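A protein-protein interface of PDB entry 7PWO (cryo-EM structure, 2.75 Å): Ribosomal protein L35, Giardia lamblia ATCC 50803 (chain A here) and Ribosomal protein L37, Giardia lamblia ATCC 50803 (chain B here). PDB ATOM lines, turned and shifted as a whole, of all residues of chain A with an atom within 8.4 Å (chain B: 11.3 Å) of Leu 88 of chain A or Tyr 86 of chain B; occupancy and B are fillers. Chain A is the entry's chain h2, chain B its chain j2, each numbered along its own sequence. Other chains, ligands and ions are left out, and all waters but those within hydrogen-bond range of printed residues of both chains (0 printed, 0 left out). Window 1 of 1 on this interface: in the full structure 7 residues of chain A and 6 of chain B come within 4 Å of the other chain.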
ATOM      1  N   ARG A  85       5.187  -3.541 -11.531  1.00  0.00           N
ATOM      2  CA  ARG A  85       5.306  -4.619 -10.566  1.00  0.00           C
ATOM      3  C   ARG A  85       6.222  -5.728 -11.085  1.00  0.00           C
ATOM      4  O   ARG A  85       6.529  -5.788 -12.277  1.00  0.00           O
ATOM      5  CB  ARG A  85       3.916  -5.156 -10.232  1.00  0.00           C
ATOM      6  CG  ARG A  85       3.090  -4.149  -9.425  1.00  0.00           C
ATOM      7  CD  ARG A  85       1.735  -4.653  -8.955  1.00  0.00           C
ATOM      8  NE  ARG A  85       0.881  -3.517  -8.620  1.00  0.00           N
ATOM      9  CZ  ARG A  85      -0.363  -3.587  -8.162  1.00  0.00           C
ATOM     10  NH1 ARG A  85      -0.957  -4.751  -7.976  1.00  0.00           N
ATOM     11  NH2 ARG A  85      -1.018  -2.476  -7.885  1.00  0.00           N
ATOM     12  N   PRO A  86       6.701  -6.598 -10.193  1.00  0.00           N
ATOM     13  CA  PRO A  86       7.573  -7.694 -10.620  1.00  0.00           C
ATOM     14  C   PRO A  86       6.938  -8.556 -11.702  1.00  0.00           C
ATOM     15  O   PRO A  86       5.714  -8.613 -11.842  1.00  0.00           O
ATOM     16  CB  PRO A  86       7.785  -8.492  -9.331  1.00  0.00           C
ATOM     17  CG  PRO A  86       7.684  -7.496  -8.277  1.00  0.00           C
ATOM     18  CD  PRO A  86       6.689  -6.466  -8.728  1.00  0.00           C
ATOM     19  N   ARG A  87       7.794  -9.219 -12.486  1.00  0.00           N
ATOM     20  CA  ARG A  87       7.336 -10.109 -13.552  1.00  0.00           C
ATOM     21  C   ARG A  87       7.228 -11.516 -12.979  1.00  0.00           C
ATOM     22  O   ARG A  87       8.231 -12.195 -12.763  1.00  0.00           O
ATOM     23  CB  ARG A  87       8.272 -10.061 -14.757  1.00  0.00           C
ATOM     24  CG  ARG A  87       7.667 -10.717 -15.994  1.00  0.00           C
ATOM     25  CD  ARG A  87       8.695 -11.313 -16.940  1.00  0.00           C
ATOM     26  NE  ARG A  87       8.041 -12.070 -18.002  1.00  0.00           N
ATOM     27  CZ  ARG A  87       8.610 -12.392 -19.159  1.00  0.00           C
ATOM     28  NH1 ARG A  87       9.850 -12.020 -19.415  1.00  0.00           N
ATOM     29  NH2 ARG A  87       7.933 -13.087 -20.059  1.00  0.00           N
ATOM     30  N   LEU A  88       5.997 -11.953 -12.737  1.00  0.00           N
ATOM     31  CA  LEU A  88       5.711 -13.201 -12.048  1.00  0.00           C
ATOM     32  C   LEU A  88       4.438 -13.782 -12.642  1.00  0.00           C
ATOM     33  O   LEU A  88       3.552 -13.039 -13.068  1.00  0.00           O
ATOM     34  CB  LEU A  88       5.511 -12.962 -10.550  1.00  0.00           C
ATOM     35  CG  LEU A  88       6.639 -12.387  -9.699  1.00  0.00           C
ATOM     36  CD1 LEU A  88       6.066 -11.984  -8.359  1.00  0.00           C
ATOM     37  CD2 LEU A  88       7.753 -13.390  -9.518  1.00  0.00           C
ATOM     38  N   THR A  89       4.338 -15.106 -12.656  1.00  0.00           N
ATOM     39  CA  THR A  89       3.100 -15.718 -13.112  1.00  0.00           C
ATOM     40  C   THR A  89       1.988 -15.523 -12.088  1.00  0.00           C
ATOM     41  O   THR A  89       2.218 -15.205 -10.918  1.00  0.00           O
ATOM     42  CB  THR A  89       3.280 -17.217 -13.398  1.00  0.00           C
ATOM     43  OG1 THR A  89       3.485 -17.933 -12.176  1.00  0.00           O
ATOM     44  CG2 THR A  89       4.433 -17.472 -14.342  1.00  0.00           C
ATOM     45  N   HIS A  90       0.761 -15.729 -12.562  1.00  0.00           N
ATOM     46  CA  HIS A  90      -0.427 -15.705 -11.719  1.00  0.00           C
ATOM     47  C   HIS A  90      -0.260 -16.607 -10.496  1.00  0.00           C
ATOM     48  O   HIS A  90      -0.523 -16.199  -9.354  1.00  0.00           O
ATOM     49  CB  HIS A  90      -1.612 -16.141 -12.581  1.00  0.00           C
ATOM     50  CG  HIS A  90      -2.952 -15.985 -11.932  1.00  0.00           C
ATOM     51  ND1 HIS A  90      -3.664 -14.808 -11.968  1.00  0.00           N
ATOM     52  CD2 HIS A  90      -3.717 -16.868 -11.249  1.00  0.00           C
ATOM     53  CE1 HIS A  90      -4.812 -14.975 -11.337  1.00  0.00           C
ATOM     54  NE2 HIS A  90      -4.867 -16.214 -10.889  1.00  0.00           N
ATOM     55  N   ALA A  91       0.211 -17.833 -10.718  1.00  0.00           N
ATOM     56  CA  ALA A  91       0.366 -18.781  -9.623  1.00  0.00           C
ATOM     57  C   ALA A  91       1.370 -18.289  -8.591  1.00  0.00           C
ATOM     58  O   ALA A  91       1.140 -18.402  -7.380  1.00  0.00           O
ATOM     59  CB  ALA A  91       0.784 -20.141 -10.175  1.00  0.00           C
ATOM     60  N   MET A  92       2.497 -17.750  -9.050  1.00  0.00           N
ATOM     61  CA  MET A  92       3.505 -17.247  -8.128  1.00  0.00           C
ATOM     62  C   MET A  92       2.965 -16.088  -7.307  1.00  0.00           C
ATOM     63  O   MET A  92       3.218 -16.001  -6.102  1.00  0.00           O
ATOM     64  CB  MET A  92       4.748 -16.811  -8.894  1.00  0.00           C
ATOM     65  CG  MET A  92       5.419 -17.904  -9.681  1.00  0.00           C
ATOM     66  SD  MET A  92       6.761 -17.214 -10.659  1.00  0.00           S
ATOM     67  CE  MET A  92       7.282 -18.628 -11.619  1.00  0.00           C
ATOM     68  N   ARG A  93       2.229 -15.177  -7.947  1.00  0.00           N
ATOM     69  CA  ARG A  93       1.625 -14.093  -7.187  1.00  0.00           C
ATOM     70  C   ARG A  93       0.685 -14.633  -6.122  1.00  0.00           C
ATOM     71  O   ARG A  93       0.531 -14.020  -5.063  1.00  0.00           O
ATOM     72  CB  ARG A  93       0.883 -13.127  -8.117  1.00  0.00           C
ATOM     73  CG  ARG A  93       1.734 -12.559  -9.244  1.00  0.00           C
ATOM     74  CD  ARG A  93       1.172 -11.278  -9.821  1.00  0.00           C
ATOM     75  NE  ARG A  93      -0.046 -11.479 -10.593  1.00  0.00           N
ATOM     76  CZ  ARG A  93      -0.090 -11.551 -11.918  1.00  0.00           C
ATOM     77  NH1 ARG A  93       1.018 -11.447 -12.619  1.00  0.00           N
ATOM     78  NH2 ARG A  93      -1.244 -11.730 -12.539  1.00  0.00           N
ATOM     79  N   CYS A  94       0.064 -15.783  -6.373  1.00  0.00           N
ATOM     80  CA  CYS A  94      -0.858 -16.342  -5.391  1.00  0.00           C
ATOM     81  C   CYS A  94      -0.222 -17.274  -4.352  1.00  0.00           C
ATOM     82  O   CYS A  94      -0.920 -17.668  -3.413  1.00  0.00           O
ATOM     83  CB  CYS A  94      -1.985 -17.087  -6.107  1.00  0.00           C
ATOM     84  SG  CYS A  94      -3.256 -15.992  -6.778  1.00  0.00           S
ATOM     85  N   GLN A  95       1.054 -17.649  -4.485  1.00  0.00           N
ATOM     86  CA  GLN A  95       1.683 -18.583  -3.544  1.00  0.00           C
ATOM     87  C   GLN A  95       2.026 -17.935  -2.199  1.00  0.00           C
ATOM     88  O   GLN A  95       2.272 -16.729  -2.111  1.00  0.00           O
ATOM     89  CB  GLN A  95       2.967 -19.167  -4.134  1.00  0.00           C
ATOM     90  CG  GLN A  95       2.786 -20.273  -5.152  1.00  0.00           C
ATOM     91  CD  GLN A  95       4.062 -20.539  -5.957  1.00  0.00           C
ATOM     92  OE1 GLN A  95       5.171 -20.242  -5.508  1.00  0.00           O
ATOM     93  NE2 GLN A  95       3.901 -21.104  -7.145  1.00  0.00           N
ATOM     94  N   LEU A  96       2.073 -18.759  -1.149  1.00  0.00           N
ATOM     95  CA  LEU A  96       2.525 -18.292   0.161  1.00  0.00           C
ATOM     96  C   LEU A  96       4.038 -18.122   0.211  1.00  0.00           C
ATOM     97  O   LEU A  96       4.789 -18.814  -0.476  1.00  0.00           O
ATOM     98  CB  LEU A  96       2.133 -19.257   1.283  1.00  0.00           C
ATOM     99  CG  LEU A  96       0.724 -19.510   1.807  1.00  0.00           C
ATOM    100  CD1 LEU A  96       0.799 -20.658   2.790  1.00  0.00           C
ATOM    101  CD2 LEU A  96       0.178 -18.277   2.500  1.00  0.00           C
ATOM    102  N   THR A  97       4.473 -17.212   1.076  1.00  0.00           N
ATOM    103  CA  THR A  97       5.883 -16.932   1.288  1.00  0.00           C
ATOM    104  C   THR A  97       6.542 -18.102   2.021  1.00  0.00           C
ATOM    105  O   THR A  97       5.887 -18.875   2.721  1.00  0.00           O
ATOM    106  CB  THR A  97       6.033 -15.619   2.071  1.00  0.00           C
ATOM    107  OG1 THR A  97       5.756 -14.517   1.205  1.00  0.00           O
ATOM    108  CG2 THR A  97       7.433 -15.429   2.626  1.00  0.00           C
ATOM    109  N   GLU A  98       7.852 -18.254   1.818  1.00  0.00           N
ATOM    110  CA  GLU A  98       8.587 -19.314   2.502  1.00  0.00           C
ATOM    111  C   GLU A  98       8.549 -19.138   4.015  1.00  0.00           C
ATOM    112  O   GLU A  98       8.448 -20.122   4.757  1.00  0.00           O
ATOM    113  CB  GLU A  98      10.027 -19.360   1.996  1.00  0.00           C
ATOM    114  CG  GLU A  98      10.179 -20.139   0.697  1.00  0.00           C
ATOM    115  CD  GLU A  98      10.346 -21.634   0.917  1.00  0.00           C
ATOM    116  OE1 GLU A  98      10.312 -22.080   2.081  1.00  0.00           O
ATOM    117  OE2 GLU A  98      10.517 -22.361  -0.084  1.00  0.00           O
ATOM    118  N   LYS A  99       8.620 -17.892   4.495  1.00  0.00           N
ATOM    119  CA  LYS A  99       8.496 -17.644   5.928  1.00  0.00           C
ATOM    120  C   LYS A  99       7.112 -18.027   6.436  1.00  0.00           C
ATOM    121  O   LYS A  99       6.978 -18.626   7.511  1.00  0.00           O
ATOM    122  CB  LYS A  99       8.776 -16.176   6.245  1.00  0.00           C
ATOM    123  CG  LYS A  99      10.185 -15.714   5.960  1.00  0.00           C
ATOM    124  CD  LYS A  99      10.479 -14.433   6.709  1.00  0.00           C
ATOM    125  CE  LYS A  99      11.877 -13.921   6.422  1.00  0.00           C
ATOM    126  NZ  LYS A  99      12.005 -13.343   5.054  1.00  0.00           N
ATOM    127  N   HIS B  66       1.790 -15.661 -25.828  1.00  0.00           N
ATOM    128  CA  HIS B  66       2.128 -15.449 -24.428  1.00  0.00           C
ATOM    129  C   HIS B  66       2.709 -16.706 -23.801  1.00  0.00           C
ATOM    130  O   HIS B  66       3.768 -16.656 -23.169  1.00  0.00           O
ATOM    131  CB  HIS B  66       0.900 -14.981 -23.647  1.00  0.00           C
ATOM    132  CG  HIS B  66       1.132 -14.890 -22.173  1.00  0.00           C
ATOM    133  ND1 HIS B  66       1.764 -13.815 -21.585  1.00  0.00           N
ATOM    134  CD2 HIS B  66       0.842 -15.749 -21.171  1.00  0.00           C
ATOM    135  CE1 HIS B  66       1.843 -14.013 -20.284  1.00  0.00           C
ATOM    136  NE2 HIS B  66       1.298 -15.181 -20.007  1.00  0.00           N
ATOM    137  N   LYS B  69       6.338 -17.344 -24.851  1.00  0.00           N
ATOM    138  CA  LYS B  69       7.319 -16.521 -24.145  1.00  0.00           C
ATOM    139  C   LYS B  69       7.486 -16.946 -22.689  1.00  0.00           C
ATOM    140  O   LYS B  69       8.612 -17.029 -22.187  1.00  0.00           O
ATOM    141  CB  LYS B  69       6.943 -15.044 -24.252  1.00  0.00           C
ATOM    142  CG  LYS B  69       7.047 -14.549 -25.670  1.00  0.00           C
ATOM    143  CD  LYS B  69       6.697 -13.092 -25.837  1.00  0.00           C
ATOM    144  CE  LYS B  69       6.929 -12.691 -27.278  1.00  0.00           C
ATOM    145  NZ  LYS B  69       5.987 -13.372 -28.212  1.00  0.00           N
ATOM    146  N   VAL B  70       6.377 -17.217 -21.991  1.00  0.00           N
ATOM    147  CA  VAL B  70       6.452 -17.583 -20.575  1.00  0.00           C
ATOM    148  C   VAL B  70       7.220 -18.889 -20.390  1.00  0.00           C
ATOM    149  O   VAL B  70       8.047 -19.011 -19.479  1.00  0.00           O
ATOM    150  CB  VAL B  70       5.046 -17.666 -19.947  1.00  0.00           C
ATOM    151  CG1 VAL B  70       5.125 -18.286 -18.564  1.00  0.00           C
ATOM    152  CG2 VAL B  70       4.429 -16.310 -19.833  1.00  0.00           C
ATOM    153  N   TYR B  71       6.961 -19.885 -21.244  1.00  0.00           N
ATOM    154  CA  TYR B  71       7.675 -21.155 -21.135  1.00  0.00           C
ATOM    155  C   TYR B  71       9.168 -20.984 -21.394  1.00  0.00           C
ATOM    156  O   TYR B  71       9.989 -21.571 -20.685  1.00  0.00           O
ATOM    157  CB  TYR B  71       7.094 -22.185 -22.102  1.00  0.00           C
ATOM    158  CG  TYR B  71       5.873 -22.930 -21.607  1.00  0.00           C
ATOM    159  CD1 TYR B  71       4.724 -22.250 -21.252  1.00  0.00           C
ATOM    160  CD2 TYR B  71       5.856 -24.313 -21.537  1.00  0.00           C
ATOM    161  CE1 TYR B  71       3.608 -22.905 -20.823  1.00  0.00           C
ATOM    162  CE2 TYR B  71       4.722 -24.989 -21.110  1.00  0.00           C
ATOM    163  CZ  TYR B  71       3.604 -24.274 -20.756  1.00  0.00           C
ATOM    164  OH  TYR B  71       2.469 -24.912 -20.321  1.00  0.00           O
ATOM    165  N   ALA B  73      10.969 -18.311 -20.945  1.00  0.00           N
ATOM    166  CA  ALA B  73      11.497 -17.586 -19.794  1.00  0.00           C
ATOM    167  C   ALA B  73      11.684 -18.503 -18.592  1.00  0.00           C
ATOM    168  O   ALA B  73      12.694 -18.414 -17.887  1.00  0.00           O
ATOM    169  CB  ALA B  73      10.570 -16.427 -19.444  1.00  0.00           C
ATOM    170  N   TYR B  74      10.722 -19.386 -18.334  1.00  0.00           N
ATOM    171  CA  TYR B  74      10.871 -20.333 -17.236  1.00  0.00           C
ATOM    172  C   TYR B  74      12.021 -21.299 -17.495  1.00  0.00           C
ATOM    173  O   TYR B  74      12.916 -21.453 -16.659  1.00  0.00           O
ATOM    174  CB  TYR B  74       9.565 -21.093 -17.023  1.00  0.00           C
ATOM    175  CG  TYR B  74       9.549 -22.008 -15.823  1.00  0.00           C
ATOM    176  CD1 TYR B  74      10.138 -23.261 -15.868  1.00  0.00           C
ATOM    177  CD2 TYR B  74       8.932 -21.621 -14.642  1.00  0.00           C
ATOM    178  CE1 TYR B  74      10.125 -24.093 -14.783  1.00  0.00           C
ATOM    179  CE2 TYR B  74       8.915 -22.455 -13.547  1.00  0.00           C
ATOM    180  CZ  TYR B  74       9.517 -23.688 -13.627  1.00  0.00           C
ATOM    181  OH  TYR B  74       9.508 -24.525 -12.548  1.00  0.00           O
ATOM    182  N   THR B  78      15.177 -15.969 -16.380  1.00  0.00           N
ATOM    183  CA  THR B  78      15.425 -15.540 -15.007  1.00  0.00           C
ATOM    184  C   THR B  78      14.186 -15.635 -14.117  1.00  0.00           C
ATOM    185  O   THR B  78      14.154 -15.049 -13.025  1.00  0.00           O
ATOM    186  CB  THR B  78      15.944 -14.107 -15.014  1.00  0.00           C
ATOM    187  OG1 THR B  78      14.923 -13.240 -15.516  1.00  0.00           O
ATOM    188  CG2 THR B  78      17.157 -14.000 -15.940  1.00  0.00           C
ATOM    189  N   LEU B  79      13.171 -16.367 -14.556  1.00  0.00           N
ATOM    190  CA  LEU B  79      11.871 -16.272 -13.911  1.00  0.00           C
ATOM    191  C   LEU B  79      11.856 -16.961 -12.548  1.00  0.00           C
ATOM    192  O   LEU B  79      11.263 -16.444 -11.597  1.00  0.00           O
ATOM    193  CB  LEU B  79      10.819 -16.859 -14.839  1.00  0.00           C
ATOM    194  CG  LEU B  79       9.384 -16.471 -14.590  1.00  0.00           C
ATOM    195  CD1 LEU B  79       9.169 -15.031 -14.998  1.00  0.00           C
ATOM    196  CD2 LEU B  79       8.519 -17.400 -15.400  1.00  0.00           C
ATOM    197  N   LYS B  80      12.496 -18.123 -12.425  1.00  0.00           N
ATOM    198  CA  LYS B  80      12.524 -18.803 -11.132  1.00  0.00           C
ATOM    199  C   LYS B  80      13.411 -18.074 -10.129  1.00  0.00           C
ATOM    200  O   LYS B  80      13.119 -18.074  -8.927  1.00  0.00           O
ATOM    201  CB  LYS B  80      12.982 -20.248 -11.315  1.00  0.00           C
ATOM    202  CG  LYS B  80      11.892 -21.173 -11.832  1.00  0.00           C
ATOM    203  CD  LYS B  80      12.413 -22.052 -12.955  1.00  0.00           C
ATOM    204  CE  LYS B  80      13.341 -23.143 -12.466  1.00  0.00           C
ATOM    205  NZ  LYS B  80      13.507 -24.214 -13.495  1.00  0.00           N
ATOM    206  N   ALA B  81      14.477 -17.422 -10.594  1.00  0.00           N
ATOM    207  CA  ALA B  81      15.205 -16.512  -9.719  1.00  0.00           C
ATOM    208  C   ALA B  81      14.299 -15.381  -9.232  1.00  0.00           C
ATOM    209  O   ALA B  81      14.334 -15.010  -8.050  1.00  0.00           O
ATOM    210  CB  ALA B  81      16.433 -15.957 -10.439  1.00  0.00           C
ATOM    211  N   ASN B  82      13.487 -14.813 -10.131  1.00  0.00           N
ATOM    212  CA  ASN B  82      12.554 -13.767  -9.712  1.00  0.00           C
ATOM    213  C   ASN B  82      11.558 -14.301  -8.695  1.00  0.00           C
ATOM    214  O   ASN B  82      11.156 -13.591  -7.766  1.00  0.00           O
ATOM    215  CB  ASN B  82      11.808 -13.204 -10.919  1.00  0.00           C
ATOM    216  CG  ASN B  82      12.503 -12.017 -11.532  1.00  0.00           C
ATOM    217  OD1 ASN B  82      13.371 -11.410 -10.921  1.00  0.00           O
ATOM    218  ND2 ASN B  82      12.121 -11.680 -12.754  1.00  0.00           N
ATOM    219  N   ALA B  83      11.140 -15.554  -8.869  1.00  0.00           N
ATOM    220  CA  ALA B  83      10.246 -16.185  -7.913  1.00  0.00           C
ATOM    221  C   ALA B  83      10.902 -16.310  -6.547  1.00  0.00           C
ATOM    222  O   ALA B  83      10.261 -16.072  -5.524  1.00  0.00           O
ATOM    223  CB  ALA B  83       9.804 -17.554  -8.428  1.00  0.00           C
ATOM    224  N   ARG B  84      12.178 -16.691  -6.507  1.00  0.00           N
ATOM    225  CA  ARG B  84      12.876 -16.767  -5.225  1.00  0.00           C
ATOM    226  C   ARG B  84      12.949 -15.395  -4.556  1.00  0.00           C
ATOM    227  O   ARG B  84      12.688 -15.260  -3.352  1.00  0.00           O
ATOM    228  CB  ARG B  84      14.274 -17.354  -5.420  1.00  0.00           C
ATOM    229  N   LYS B  85      13.276 -14.357  -5.329  1.00  0.00           N
ATOM    230  CA  LYS B  85      13.330 -13.009  -4.761  1.00  0.00           C
ATOM    231  C   LYS B  85      11.969 -12.575  -4.210  1.00  0.00           C
ATOM    232  O   LYS B  85      11.892 -11.969  -3.135  1.00  0.00           O
ATOM    233  CB  LYS B  85      13.828 -12.010  -5.804  1.00  0.00           C
ATOM    234  N   TYR B  86      10.888 -12.871  -4.929  1.00  0.00           N
ATOM    235  CA  TYR B  86       9.555 -12.540  -4.425  1.00  0.00           C
ATOM    236  C   TYR B  86       9.217 -13.337  -3.171  1.00  0.00           C
ATOM    237  O   TYR B  86       8.735 -12.779  -2.180  1.00  0.00           O
ATOM    238  CB  TYR B  86       8.503 -12.800  -5.501  1.00  0.00           C
ATOM    239  CG  TYR B  86       7.126 -12.266  -5.179  1.00  0.00           C
ATOM    240  CD1 TYR B  86       6.921 -10.918  -4.886  1.00  0.00           C
ATOM    241  CD2 TYR B  86       6.029 -13.117  -5.138  1.00  0.00           C
ATOM    242  CE1 TYR B  86       5.664 -10.435  -4.598  1.00  0.00           C
ATOM    243  CE2 TYR B  86       4.767 -12.645  -4.837  1.00  0.00           C
ATOM    244  CZ  TYR B  86       4.589 -11.304  -4.571  1.00  0.00           C
ATOM    245  OH  TYR B  86       3.327 -10.835  -4.275  1.00  0.00           O
ATOM    246  N   LEU B  87       9.474 -14.640  -3.189  1.00  0.00           N
ATOM    247  CA  LEU B  87       9.030 -15.528  -2.126  1.00  0.00           C
ATOM    248  C   LEU B  87       9.944 -15.497  -0.914  1.00  0.00           C
ATOM    249  O   LEU B  87       9.682 -16.217   0.054  1.00  0.00           O
ATOM    250  CB  LEU B  87       8.906 -16.964  -2.647  1.00  0.00           C
ATOM    251  CG  LEU B  87       7.589 -17.280  -3.380  1.00  0.00           C
ATOM    252  CD1 LEU B  87       6.427 -17.150  -2.435  1.00  0.00           C
ATOM    253  CD2 LEU B  87       7.350 -16.427  -4.620  1.00  0.00           C
ATOM    254  N   ALA B  88      11.010 -14.707  -0.953  1.00  0.00           N
ATOM    255  CA  ALA B  88      11.779 -14.410   0.247  1.00  0.00           C
ATOM    256  C   ALA B  88      10.902 -13.730   1.291  1.00  0.00           C
ATOM    257  O   ALA B  88      10.642 -12.523   1.219  1.00  0.00           O
ATOM    258  CB  ALA B  88      12.968 -13.539  -0.088  1.00  0.00           C
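The backbone NH of Glu 98 of chain A is in hydrogen-bond range of the backbone carbonyl oxygen of Leu 87 of chain B (3.3 Å).
Arg 87 of chain A touches Leu 79 of chain B (O to CD1, 3.7 Å). ND2 of Asn 82 of chain B touches O of Arg 87 of chain A (3.9 Å). Asn 82 of chain B touches Leu 88 of chain A (O to CD2, 3.8 Å). Leu 88 of chain A touches Tyr 86 of chain B (CD1 to CG, 3.4 Å). SD of Met 92 of chain A touches CB of Ala 83 of chain B, 3.8 Å away. CE2 of Tyr 86 of chain B touches O of Met 92 of chain A, at 3.9 Å. CD1 of Leu 87 of chain B touches O of Leu 96 of chain A, at 3.0 Å. Thr 97 of chain A touches Leu 87 of chain B. C of Ala 88 of chain B touches NZ of Lys 99 of chain A, 3.9 Å away.
Printed residues of chain B that touch a printed residue of chain A: Leu 79, Asn 82, Ala 83, Tyr 86, Leu 87 and Ala 88. Hydrophobic or aromatic side chains of chain B within 4 Å of the printed part of chain A: Leu 79, Ala 83, Tyr 86 and Leu 87. Printed residues of chain A that touch a printed residue of chain B: Arg 87, Leu 88, Met 92, Leu 96, Thr 97, Glu 98 and Lys 99. Hydrophobic or aromatic side chains of chain A within 4 Å of the printed part of chain B: Leu 88 and Met 92.
The backbone NH of Met 92 of chain A sits close to the side-chain hydroxyl of Thr 89 of chain A, 3.3 Å away. O of Leu 88 of chain A lies within hydrogen-bond range of NH1 of Arg 93 of chain A (3.0 Å).
Thr 89 of chain A touches none of the printed residues of chain B. Of chain B, only Ala 83 and Tyr 86 come within 4 Å of Met 92 of chain A. Printed residues of chain B within 4 Å of Leu 96 of chain A: Leu 87 (3.0 Å). Of the printed residues of chain B, Thr 97 of chain A touches Leu 87 (3.5 Å). Printed residues of chain A within 4 Å of Ala 83 of chain B: Met 92. Lys 85 of chain B touches none of the printed residues of chain A. Of the printed residues of chain A, Leu 87 of chain B touches Leu 96, Thr 97 and Glu 98. The nearest printed residue of chain A that does not touch Ala 88 of chain B is Thr 97 of chain A (4.1 Å).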
